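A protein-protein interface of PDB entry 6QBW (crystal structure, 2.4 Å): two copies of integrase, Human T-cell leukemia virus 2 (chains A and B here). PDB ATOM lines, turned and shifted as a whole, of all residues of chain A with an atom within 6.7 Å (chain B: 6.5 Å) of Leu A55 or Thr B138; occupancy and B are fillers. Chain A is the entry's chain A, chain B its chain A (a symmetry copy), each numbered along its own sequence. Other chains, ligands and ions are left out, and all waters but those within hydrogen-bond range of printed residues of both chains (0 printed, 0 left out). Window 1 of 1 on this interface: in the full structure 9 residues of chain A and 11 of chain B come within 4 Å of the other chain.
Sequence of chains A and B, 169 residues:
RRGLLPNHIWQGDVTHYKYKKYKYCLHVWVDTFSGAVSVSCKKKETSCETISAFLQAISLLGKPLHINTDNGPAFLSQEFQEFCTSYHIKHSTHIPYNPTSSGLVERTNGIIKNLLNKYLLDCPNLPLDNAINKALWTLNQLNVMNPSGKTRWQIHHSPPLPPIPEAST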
ATOM      1  N   TRP A  29      29.093 -40.101  16.476  1.00  0.00           N
ATOM      2  CA  TRP A  29      27.738 -39.902  16.002  1.00  0.00           C
ATOM      3  C   TRP A  29      27.494 -40.798  14.803  1.00  0.00           C
ATOM      4  O   TRP A  29      28.160 -40.652  13.780  1.00  0.00           O
ATOM      5  CB  TRP A  29      27.527 -38.437  15.624  1.00  0.00           C
ATOM      6  CG  TRP A  29      27.655 -37.524  16.796  1.00  0.00           C
ATOM      7  CD1 TRP A  29      28.758 -36.807  17.165  1.00  0.00           C
ATOM      8  CD2 TRP A  29      26.650 -37.247  17.776  1.00  0.00           C
ATOM      9  NE1 TRP A  29      28.497 -36.089  18.310  1.00  0.00           N
ATOM     10  CE2 TRP A  29      27.208 -36.341  18.704  1.00  0.00           C
ATOM     11  CE3 TRP A  29      25.330 -37.673  17.956  1.00  0.00           C
ATOM     12  CZ2 TRP A  29      26.492 -35.856  19.799  1.00  0.00           C
ATOM     13  CZ3 TRP A  29      24.618 -37.193  19.044  1.00  0.00           C
ATOM     14  CH2 TRP A  29      25.200 -36.293  19.953  1.00  0.00           C
ATOM     15  N   THR A  50      31.662 -30.994  23.197  1.00  0.00           N
ATOM     16  CA  THR A  50      30.511 -31.840  22.881  1.00  0.00           C
ATOM     17  C   THR A  50      29.672 -31.226  21.763  1.00  0.00           C
ATOM     18  O   THR A  50      29.280 -31.922  20.822  1.00  0.00           O
ATOM     19  CB  THR A  50      29.621 -32.056  24.122  1.00  0.00           C
ATOM     20  OG1 THR A  50      30.440 -32.414  25.238  1.00  0.00           O
ATOM     21  CG2 THR A  50      28.587 -33.157  23.879  1.00  0.00           C
ATOM     22  N   ILE A  51      29.400 -29.924  21.881  1.00  0.00           N
ATOM     23  CA  ILE A  51      28.670 -29.187  20.852  1.00  0.00           C
ATOM     24  C   ILE A  51      29.537 -29.085  19.602  1.00  0.00           C
ATOM     25  O   ILE A  51      29.040 -29.248  18.492  1.00  0.00           O
ATOM     26  CB  ILE A  51      28.234 -27.781  21.339  1.00  0.00           C
ATOM     27  CG1 ILE A  51      27.191 -27.905  22.452  1.00  0.00           C
ATOM     28  CG2 ILE A  51      27.650 -26.952  20.196  1.00  0.00           C
ATOM     29  CD1 ILE A  51      26.919 -26.608  23.186  1.00  0.00           C
ATOM     30  N   SER A  52      30.830 -28.835  19.780  1.00  0.00           N
ATOM     31  CA  SER A  52      31.750 -28.771  18.645  1.00  0.00           C
ATOM     32  C   SER A  52      31.833 -30.085  17.868  1.00  0.00           C
ATOM     33  O   SER A  52      31.897 -30.080  16.637  1.00  0.00           O
ATOM     34  CB  SER A  52      33.148 -28.366  19.097  1.00  0.00           C
ATOM     35  OG  SER A  52      34.002 -28.267  17.973  1.00  0.00           O
ATOM     36  N   ALA A  53      31.835 -31.204  18.585  1.00  0.00           N
ATOM     37  CA  ALA A  53      31.847 -32.521  17.948  1.00  0.00           C
ATOM     38  C   ALA A  53      30.520 -32.799  17.243  1.00  0.00           C
ATOM     39  O   ALA A  53      30.480 -33.433  16.188  1.00  0.00           O
ATOM     40  CB  ALA A  53      32.137 -33.596  18.979  1.00  0.00           C
ATOM     41  N   PHE A  54      29.437 -32.314  17.833  1.00  0.00           N
ATOM     42  CA  PHE A  54      28.100 -32.511  17.278  1.00  0.00           C
ATOM     43  C   PHE A  54      27.883 -31.690  15.999  1.00  0.00           C
ATOM     44  O   PHE A  54      27.332 -32.192  15.019  1.00  0.00           O
ATOM     45  CB  PHE A  54      27.050 -32.172  18.348  1.00  0.00           C
ATOM     46  CG  PHE A  54      25.636 -32.516  17.964  1.00  0.00           C
ATOM     47  CD1 PHE A  54      25.340 -33.679  17.261  1.00  0.00           C
ATOM     48  CD2 PHE A  54      24.593 -31.686  18.337  1.00  0.00           C
ATOM     49  CE1 PHE A  54      24.031 -33.989  16.922  1.00  0.00           C
ATOM     50  CE2 PHE A  54      23.289 -31.995  18.005  1.00  0.00           C
ATOM     51  CZ  PHE A  54      23.006 -33.147  17.297  1.00  0.00           C
ATOM     52  N   LEU A  55      28.321 -30.434  16.017  1.00  0.00           N
ATOM     53  CA  LEU A  55      28.231 -29.572  14.840  1.00  0.00           C
ATOM     54  C   LEU A  55      29.004 -30.171  13.675  1.00  0.00           C
ATOM     55  O   LEU A  55      28.530 -30.159  12.540  1.00  0.00           O
ATOM     56  CB  LEU A  55      28.774 -28.172  15.136  1.00  0.00           C
ATOM     57  CG  LEU A  55      27.817 -27.162  15.760  1.00  0.00           C
ATOM     58  CD1 LEU A  55      28.590 -25.970  16.301  1.00  0.00           C
ATOM     59  CD2 LEU A  55      26.784 -26.717  14.738  1.00  0.00           C
ATOM     60  N   GLN A  56      30.196 -30.683  13.967  1.00  0.00           N
ATOM     61  CA  GLN A  56      31.012 -31.355  12.964  1.00  0.00           C
ATOM     62  C   GLN A  56      30.310 -32.560  12.346  1.00  0.00           C
ATOM     63  O   GLN A  56      30.436 -32.800  11.149  1.00  0.00           O
ATOM     64  CB  GLN A  56      32.337 -31.805  13.563  1.00  0.00           C
ATOM     65  CG  GLN A  56      33.250 -32.459  12.543  1.00  0.00           C
ATOM     66  CD  GLN A  56      34.701 -32.187  12.834  1.00  0.00           C
ATOM     67  OE1 GLN A  56      35.229 -32.609  13.866  1.00  0.00           O
ATOM     68  NE2 GLN A  56      35.356 -31.460  11.933  1.00  0.00           N
ATOM     69  N   ALA A  57      29.595 -33.322  13.166  1.00  0.00           N
ATOM     70  CA  ALA A  57      28.817 -34.451  12.678  1.00  0.00           C
ATOM     71  C   ALA A  57      27.681 -33.979  11.772  1.00  0.00           C
ATOM     72  O   ALA A  57      27.395 -34.598  10.748  1.00  0.00           O
ATOM     73  CB  ALA A  57      28.267 -35.253  13.845  1.00  0.00           C
ATOM     74  N   ILE A  58      27.041 -32.879  12.154  1.00  0.00           N
ATOM     75  CA  ILE A  58      26.004 -32.267  11.331  1.00  0.00           C
ATOM     76  C   ILE A  58      26.610 -31.701  10.042  1.00  0.00           C
ATOM     77  O   ILE A  58      26.016 -31.811   8.967  1.00  0.00           O
ATOM     78  CB  ILE A  58      25.245 -31.174  12.115  1.00  0.00           C
ATOM     79  CG1 ILE A  58      24.456 -31.817  13.260  1.00  0.00           C
ATOM     80  CG2 ILE A  58      24.295 -30.406  11.204  1.00  0.00           C
ATOM     81  CD1 ILE A  58      23.993 -30.838  14.314  1.00  0.00           C
ATOM     82  N   SER A  59      27.792 -31.107  10.162  1.00  0.00           N
ATOM     83  CA  SER A  59      28.562 -30.630   9.007  1.00  0.00           C
ATOM     84  C   SER A  59      28.771 -31.695   7.916  1.00  0.00           C
ATOM     85  O   SER A  59      28.656 -31.402   6.727  1.00  0.00           O
ATOM     86  CB  SER A  59      29.916 -30.081   9.484  1.00  0.00           C
ATOM     87  OG  SER A  59      30.981 -30.442   8.626  1.00  0.00           O
ATOM     88  N   LEU A  60      29.074 -32.921   8.337  1.00  0.00           N
ATOM     89  CA  LEU A  60      29.351 -34.037   7.426  1.00  0.00           C
ATOM     90  C   LEU A  60      28.101 -34.830   7.016  1.00  0.00           C
ATOM     91  O   LEU A  60      28.027 -35.329   5.891  1.00  0.00           O
ATOM     92  CB  LEU A  60      30.365 -34.993   8.068  1.00  0.00           C
ATOM     93  CG  LEU A  60      31.844 -34.694   7.791  1.00  0.00           C
ATOM     94  CD1 LEU A  60      32.715 -34.912   9.026  1.00  0.00           C
ATOM     95  CD2 LEU A  60      32.334 -35.551   6.626  1.00  0.00           C
ATOM     96  N   PHE A  83      21.248 -26.217  23.537  1.00  0.00           N
ATOM     97  CA  PHE A  83      21.651 -26.242  22.138  1.00  0.00           C
ATOM     98  C   PHE A  83      20.639 -27.019  21.304  1.00  0.00           C
ATOM     99  O   PHE A  83      20.184 -26.536  20.270  1.00  0.00           O
ATOM    100  CB  PHE A  83      23.047 -26.853  21.961  1.00  0.00           C
ATOM    101  CG  PHE A  83      23.473 -26.963  20.524  1.00  0.00           C
ATOM    102  CD1 PHE A  83      24.100 -25.903  19.890  1.00  0.00           C
ATOM    103  CD2 PHE A  83      23.217 -28.117  19.796  1.00  0.00           C
ATOM    104  CE1 PHE A  83      24.478 -25.996  18.564  1.00  0.00           C
ATOM    105  CE2 PHE A  83      23.592 -28.217  18.469  1.00  0.00           C
ATOM    106  CZ  PHE A  83      24.225 -27.155  17.855  1.00  0.00           C
ATOM    107  N   TYR A  87      17.787 -25.515  18.211  1.00  0.00           N
ATOM    108  CA  TYR A  87      17.809 -25.861  16.788  1.00  0.00           C
ATOM    109  C   TYR A  87      16.889 -27.029  16.441  1.00  0.00           C
ATOM    110  O   TYR A  87      17.111 -27.720  15.453  1.00  0.00           O
ATOM    111  CB  TYR A  87      19.260 -26.109  16.333  1.00  0.00           C
ATOM    112  CG  TYR A  87      20.096 -24.854  16.465  1.00  0.00           C
ATOM    113  CD1 TYR A  87      19.996 -23.831  15.528  1.00  0.00           C
ATOM    114  CD2 TYR A  87      20.938 -24.663  17.551  1.00  0.00           C
ATOM    115  CE1 TYR A  87      20.728 -22.669  15.660  1.00  0.00           C
ATOM    116  CE2 TYR A  87      21.674 -23.502  17.688  1.00  0.00           C
ATOM    117  CZ  TYR A  87      21.565 -22.507  16.739  1.00  0.00           C
ATOM    118  OH  TYR A  87      22.294 -21.346  16.871  1.00  0.00           O
ATOM    119  N   LEU B 115      27.157 -14.987  15.612  1.00  0.00           N
ATOM    120  CA  LEU B 115      27.564 -16.354  15.938  1.00  0.00           C
ATOM    121  C   LEU B 115      29.018 -16.432  16.400  1.00  0.00           C
ATOM    122  O   LEU B 115      29.329 -17.174  17.329  1.00  0.00           O
ATOM    123  CB  LEU B 115      27.335 -17.289  14.749  1.00  0.00           C
ATOM    124  CG  LEU B 115      25.868 -17.657  14.519  1.00  0.00           C
ATOM    125  CD1 LEU B 115      25.611 -18.054  13.074  1.00  0.00           C
ATOM    126  CD2 LEU B 115      25.439 -18.768  15.465  1.00  0.00           C
ATOM    127  N   LYS B 118      29.216 -15.160  19.915  1.00  0.00           N
ATOM    128  CA  LYS B 118      28.620 -16.150  20.801  1.00  0.00           C
ATOM    129  C   LYS B 118      29.560 -17.326  21.031  1.00  0.00           C
ATOM    130  O   LYS B 118      29.807 -17.707  22.173  1.00  0.00           O
ATOM    131  CB  LYS B 118      27.290 -16.658  20.240  1.00  0.00           C
ATOM    132  CG  LYS B 118      26.397 -17.327  21.278  1.00  0.00           C
ATOM    133  CD  LYS B 118      25.319 -18.193  20.632  1.00  0.00           C
ATOM    134  CE  LYS B 118      25.856 -19.571  20.258  1.00  0.00           C
ATOM    135  NZ  LYS B 118      24.892 -20.383  19.457  1.00  0.00           N
ATOM    136  N   TYR B 119      30.088 -17.901  19.956  1.00  0.00           N
ATOM    137  CA  TYR B 119      30.970 -19.062  20.093  1.00  0.00           C
ATOM    138  C   TYR B 119      32.275 -18.730  20.818  1.00  0.00           C
ATOM    139  O   TYR B 119      32.778 -19.548  21.583  1.00  0.00           O
ATOM    140  CB  TYR B 119      31.232 -19.734  18.738  1.00  0.00           C
ATOM    141  CG  TYR B 119      30.069 -20.590  18.262  1.00  0.00           C
ATOM    142  CD1 TYR B 119      29.530 -21.581  19.084  1.00  0.00           C
ATOM    143  CD2 TYR B 119      29.511 -20.415  16.999  1.00  0.00           C
ATOM    144  CE1 TYR B 119      28.468 -22.363  18.669  1.00  0.00           C
ATOM    145  CE2 TYR B 119      28.449 -21.199  16.574  1.00  0.00           C
ATOM    146  CZ  TYR B 119      27.932 -22.171  17.417  1.00  0.00           C
ATOM    147  OH  TYR B 119      26.878 -22.956  17.018  1.00  0.00           O
ATOM    148  N   ASN B 133      34.262 -22.092  11.881  1.00  0.00           N
ATOM    149  CA  ASN B 133      33.665 -23.358  11.444  1.00  0.00           C
ATOM    150  C   ASN B 133      32.308 -23.558  12.106  1.00  0.00           C
ATOM    151  O   ASN B 133      31.315 -23.825  11.437  1.00  0.00           O
ATOM    152  CB  ASN B 133      34.580 -24.546  11.761  1.00  0.00           C
ATOM    153  CG  ASN B 133      35.807 -24.591  10.876  1.00  0.00           C
ATOM    154  OD1 ASN B 133      35.782 -24.149   9.728  1.00  0.00           O
ATOM    155  ND2 ASN B 133      36.889 -25.134  11.406  1.00  0.00           N
ATOM    156  N   LYS B 134      32.273 -23.398  13.424  1.00  0.00           N
ATOM    157  CA  LYS B 134      31.045 -23.569  14.177  1.00  0.00           C
ATOM    158  C   LYS B 134      29.965 -22.599  13.681  1.00  0.00           C
ATOM    159  O   LYS B 134      28.811 -22.986  13.522  1.00  0.00           O
ATOM    160  CB  LYS B 134      31.309 -23.407  15.675  1.00  0.00           C
ATOM    161  CG  LYS B 134      32.171 -24.521  16.254  1.00  0.00           C
ATOM    162  CD  LYS B 134      32.604 -24.261  17.698  1.00  0.00           C
ATOM    163  CE  LYS B 134      31.563 -24.752  18.703  1.00  0.00           C
ATOM    164  NZ  LYS B 134      32.074 -24.907  20.098  1.00  0.00           N
ATOM    165  N   ALA B 135      30.351 -21.357  13.404  1.00  0.00           N
ATOM    166  CA  ALA B 135      29.418 -20.361  12.889  1.00  0.00           C
ATOM    167  C   ALA B 135      28.900 -20.718  11.498  1.00  0.00           C
ATOM    168  O   ALA B 135      27.702 -20.591  11.229  1.00  0.00           O
ATOM    169  CB  ALA B 135      30.072 -18.992  12.863  1.00  0.00           C
ATOM    170  N   LEU B 136      29.801 -21.147  10.613  1.00  0.00           N
ATOM    171  CA  LEU B 136      29.420 -21.531   9.245  1.00  0.00           C
ATOM    172  C   LEU B 136      28.482 -22.731   9.244  1.00  0.00           C
ATOM    173  O   LEU B 136      27.448 -22.728   8.563  1.00  0.00           O
ATOM    174  CB  LEU B 136      30.650 -21.868   8.396  1.00  0.00           C
ATOM    175  CG  LEU B 136      31.402 -20.710   7.738  1.00  0.00           C
ATOM    176  CD1 LEU B 136      32.626 -21.226   6.994  1.00  0.00           C
ATOM    177  CD2 LEU B 136      30.493 -19.945   6.790  1.00  0.00           C
ATOM    178  N   TRP B 137      28.853 -23.756  10.006  1.00  0.00           N
ATOM    179  CA  TRP B 137      28.063 -24.978  10.096  1.00  0.00           C
ATOM    180  C   TRP B 137      26.684 -24.725  10.699  1.00  0.00           C
ATOM    181  O   TRP B 137      25.712 -25.369  10.308  1.00  0.00           O
ATOM    182  CB  TRP B 137      28.789 -26.043  10.928  1.00  0.00           C
ATOM    183  CG  TRP B 137      30.113 -26.493  10.372  1.00  0.00           C
ATOM    184  CD1 TRP B 137      30.518 -26.457   9.070  1.00  0.00           C
ATOM    185  CD2 TRP B 137      31.194 -27.077  11.112  1.00  0.00           C
ATOM    186  NE1 TRP B 137      31.786 -26.965   8.955  1.00  0.00           N
ATOM    187  CE2 TRP B 137      32.225 -27.357  10.193  1.00  0.00           C
ATOM    188  CE3 TRP B 137      31.387 -27.393  12.466  1.00  0.00           C
ATOM    189  CZ2 TRP B 137      33.440 -27.936  10.580  1.00  0.00           C
ATOM    190  CZ3 TRP B 137      32.594 -27.971  12.855  1.00  0.00           C
ATOM    191  CH2 TRP B 137      33.605 -28.238  11.912  1.00  0.00           C
ATOM    192  N   THR B 138      26.603 -23.803  11.659  1.00  0.00           N
ATOM    193  CA  THR B 138      25.323 -23.457  12.277  1.00  0.00           C
ATOM    194  C   THR B 138      24.427 -22.734  11.269  1.00  0.00           C
ATOM    195  O   THR B 138      23.228 -22.998  11.182  1.00  0.00           O
ATOM    196  CB  THR B 138      25.499 -22.567  13.525  1.00  0.00           C
ATOM    197  OG1 THR B 138      26.321 -23.234  14.488  1.00  0.00           O
ATOM    198  CG2 THR B 138      24.153 -22.255  14.161  1.00  0.00           C
ATOM    199  N   LEU B 139      25.025 -21.827  10.506  1.00  0.00           N
ATOM    200  CA  LEU B 139      24.276 -21.012   9.572  1.00  0.00           C
ATOM    201  C   LEU B 139      23.801 -21.835   8.383  1.00  0.00           C
ATOM    202  O   LEU B 139      22.615 -21.840   8.062  1.00  0.00           O
ATOM    203  CB  LEU B 139      25.132 -19.837   9.094  1.00  0.00           C
ATOM    204  CG  LEU B 139      24.433 -18.778   8.245  1.00  0.00           C
ATOM    205  CD1 LEU B 139      23.145 -18.339   8.918  1.00  0.00           C
ATOM    206  CD2 LEU B 139      25.358 -17.595   8.017  1.00  0.00           C
ATOM    207  N   ASN B 140      24.723 -22.544   7.741  1.00  0.00           N
ATOM    208  CA  ASN B 140      24.390 -23.270   6.517  1.00  0.00           C
ATOM    209  C   ASN B 140      23.511 -24.498   6.742  1.00  0.00           C
ATOM    210  O   ASN B 140      22.566 -24.728   5.981  1.00  0.00           O
ATOM    211  CB  ASN B 140      25.664 -23.676   5.769  1.00  0.00           C
ATOM    212  CG  ASN B 140      26.345 -22.504   5.094  1.00  0.00           C
ATOM    213  OD1 ASN B 140      25.685 -21.623   4.547  1.00  0.00           O
ATOM    214  ND2 ASN B 140      27.677 -22.494   5.116  1.00  0.00           N
ATOM    215  N   GLN B 141      23.814 -25.274   7.782  1.00  0.00           N
ATOM    216  CA  GLN B 141      23.254 -26.623   7.929  1.00  0.00           C
ATOM    217  C   GLN B 141      22.395 -26.844   9.175  1.00  0.00           C
ATOM    218  O   GLN B 141      21.713 -27.866   9.282  1.00  0.00           O
ATOM    219  CB  GLN B 141      24.389 -27.644   7.879  1.00  0.00           C
ATOM    220  CG  GLN B 141      25.438 -27.240   6.858  1.00  0.00           C
ATOM    221  CD  GLN B 141      26.413 -28.333   6.509  1.00  0.00           C
ATOM    222  OE1 GLN B 141      26.021 -29.475   6.244  1.00  0.00           O
ATOM    223  NE2 GLN B 141      27.705 -27.984   6.479  1.00  0.00           N
ATOM    224  N   LEU B 142      22.399 -25.895  10.102  1.00  0.00           N
ATOM    225  CA  LEU B 142      21.613 -26.045  11.313  1.00  0.00           C
ATOM    226  C   LEU B 142      20.382 -25.144  11.318  1.00  0.00           C
ATOM    227  O   LEU B 142      19.298 -25.583  11.712  1.00  0.00           O
ATOM    228  CB  LEU B 142      22.485 -25.776  12.531  1.00  0.00           C
ATOM    229  CG  LEU B 142      22.022 -26.408  13.834  1.00  0.00           C
ATOM    230  CD1 LEU B 142      21.816 -27.910  13.703  1.00  0.00           C
ATOM    231  CD2 LEU B 142      23.047 -26.095  14.908  1.00  0.00           C
ATOM    232  N   ASN B 143      20.545 -23.894  10.886  1.00  0.00           N
ATOM    233  CA  ASN B 143      19.418 -22.965  10.793  1.00  0.00           C
ATOM    234  C   ASN B 143      18.420 -23.435   9.745  1.00  0.00           C
ATOM    235  O   ASN B 143      18.771 -23.620   8.586  1.00  0.00           O
ATOM    236  CB  ASN B 143      19.889 -21.550  10.443  1.00  0.00           C
ATOM    237  CG  ASN B 143      20.633 -20.880  11.581  1.00  0.00           C
ATOM    238  OD1 ASN B 143      21.138 -21.540  12.486  1.00  0.00           O
ATOM    239  ND2 ASN B 143      20.708 -19.557  11.535  1.00  0.00           N
ATOM    240  N   VAL B 144      17.178 -23.634  10.169  1.00  0.00           N
ATOM    241  CA  VAL B 144      16.098 -24.000   9.261  1.00  0.00           C
ATOM    242  C   VAL B 144      15.438 -22.720   8.760  1.00  0.00           C
ATOM    243  O   VAL B 144      14.883 -21.949   9.538  1.00  0.00           O
ATOM    244  CB  VAL B 144      15.060 -24.919   9.945  1.00  0.00           C
ATOM    245  CG1 VAL B 144      13.774 -24.993   9.130  1.00  0.00           C
ATOM    246  CG2 VAL B 144      15.644 -26.310  10.158  1.00  0.00           C
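OE1 of Gln B141 sits close to O of Ser A59, 3.3 Å away.
The backbone carbonyl oxygen (O) of Gln A56 sits close to the side-chain hydroxyl (OG) of Ser A59 (3.5 Å).
The backbone carbonyl oxygen of Lys B134 sits at hydrogen-bond distance from the side-chain hydroxyl of Thr B138 (2.7 Å).
OH of Tyr B119 sits at hydrogen-bond distance from OG1 of Thr B138, at 2.6 Å.
N of Leu B142 sits at hydrogen-bond distance from O of Trp B137, 3.4 Å away.
N of Asn B143 lies within hydrogen-bond range of O of Thr B138 (2.8 Å).
CD1 of Leu A55 touches OH of Tyr B119, at 3.5 Å.
Leu A55 touches Lys B134.
Trp B137 touches Gln A56.
O of Ile A58 touches OE1 of Gln B141 (3.6 Å).
CD1 of Leu B142 touches CD1 of Ile A58, at 3.7 Å.
Ser A59 touches Trp B137.
Phe A83 touches Leu B142.
Thr B138 touches Tyr A87.
Tyr A87 touches Leu B142 (CG to CD2, 3.6 Å).
Tyr A87 touches Asn B143 (CE1 to OD1, 3.4 Å).
Of the printed residues of chain B, Leu A55 touches Tyr B119 (3.5 Å), Lys B134 (3.8 Å), Trp B137 (3.8 Å), Thr B138 (3.5 Å) and Leu B142 (3.8 Å).
Of chain A, only Leu A55 and Tyr A87 come within 4 Å of Thr B138.
Printed residues of chain B within 4 Å of Phe A83: Leu B142 (3.3 Å).
Of the printed residues of chain A, Tyr B119 touches Leu A55.
Printed residues of chain B within 4 Å of Ile A58: Gln B141 and Leu B142.
Thr A50 touches none of the printed residues of chain B.
The nearest residue of chain B that does not touch Leu A55 is Ala B135 (5.7 Å).
Hydrophobic or aromatic side chains of chain A that line the printed part of chain B: Leu A55, Ile A58, Phe A83 and Tyr A87.
Among the printed residues, no Asp or Glu carboxylate lies within 4 Å of a Lys or Arg side-chain nitrogen of the other chain.
No position is printed for both chains.
Of the 16 pairs that touch across the chains among the printed residues, none has its exchanged pair printed and touching as well.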
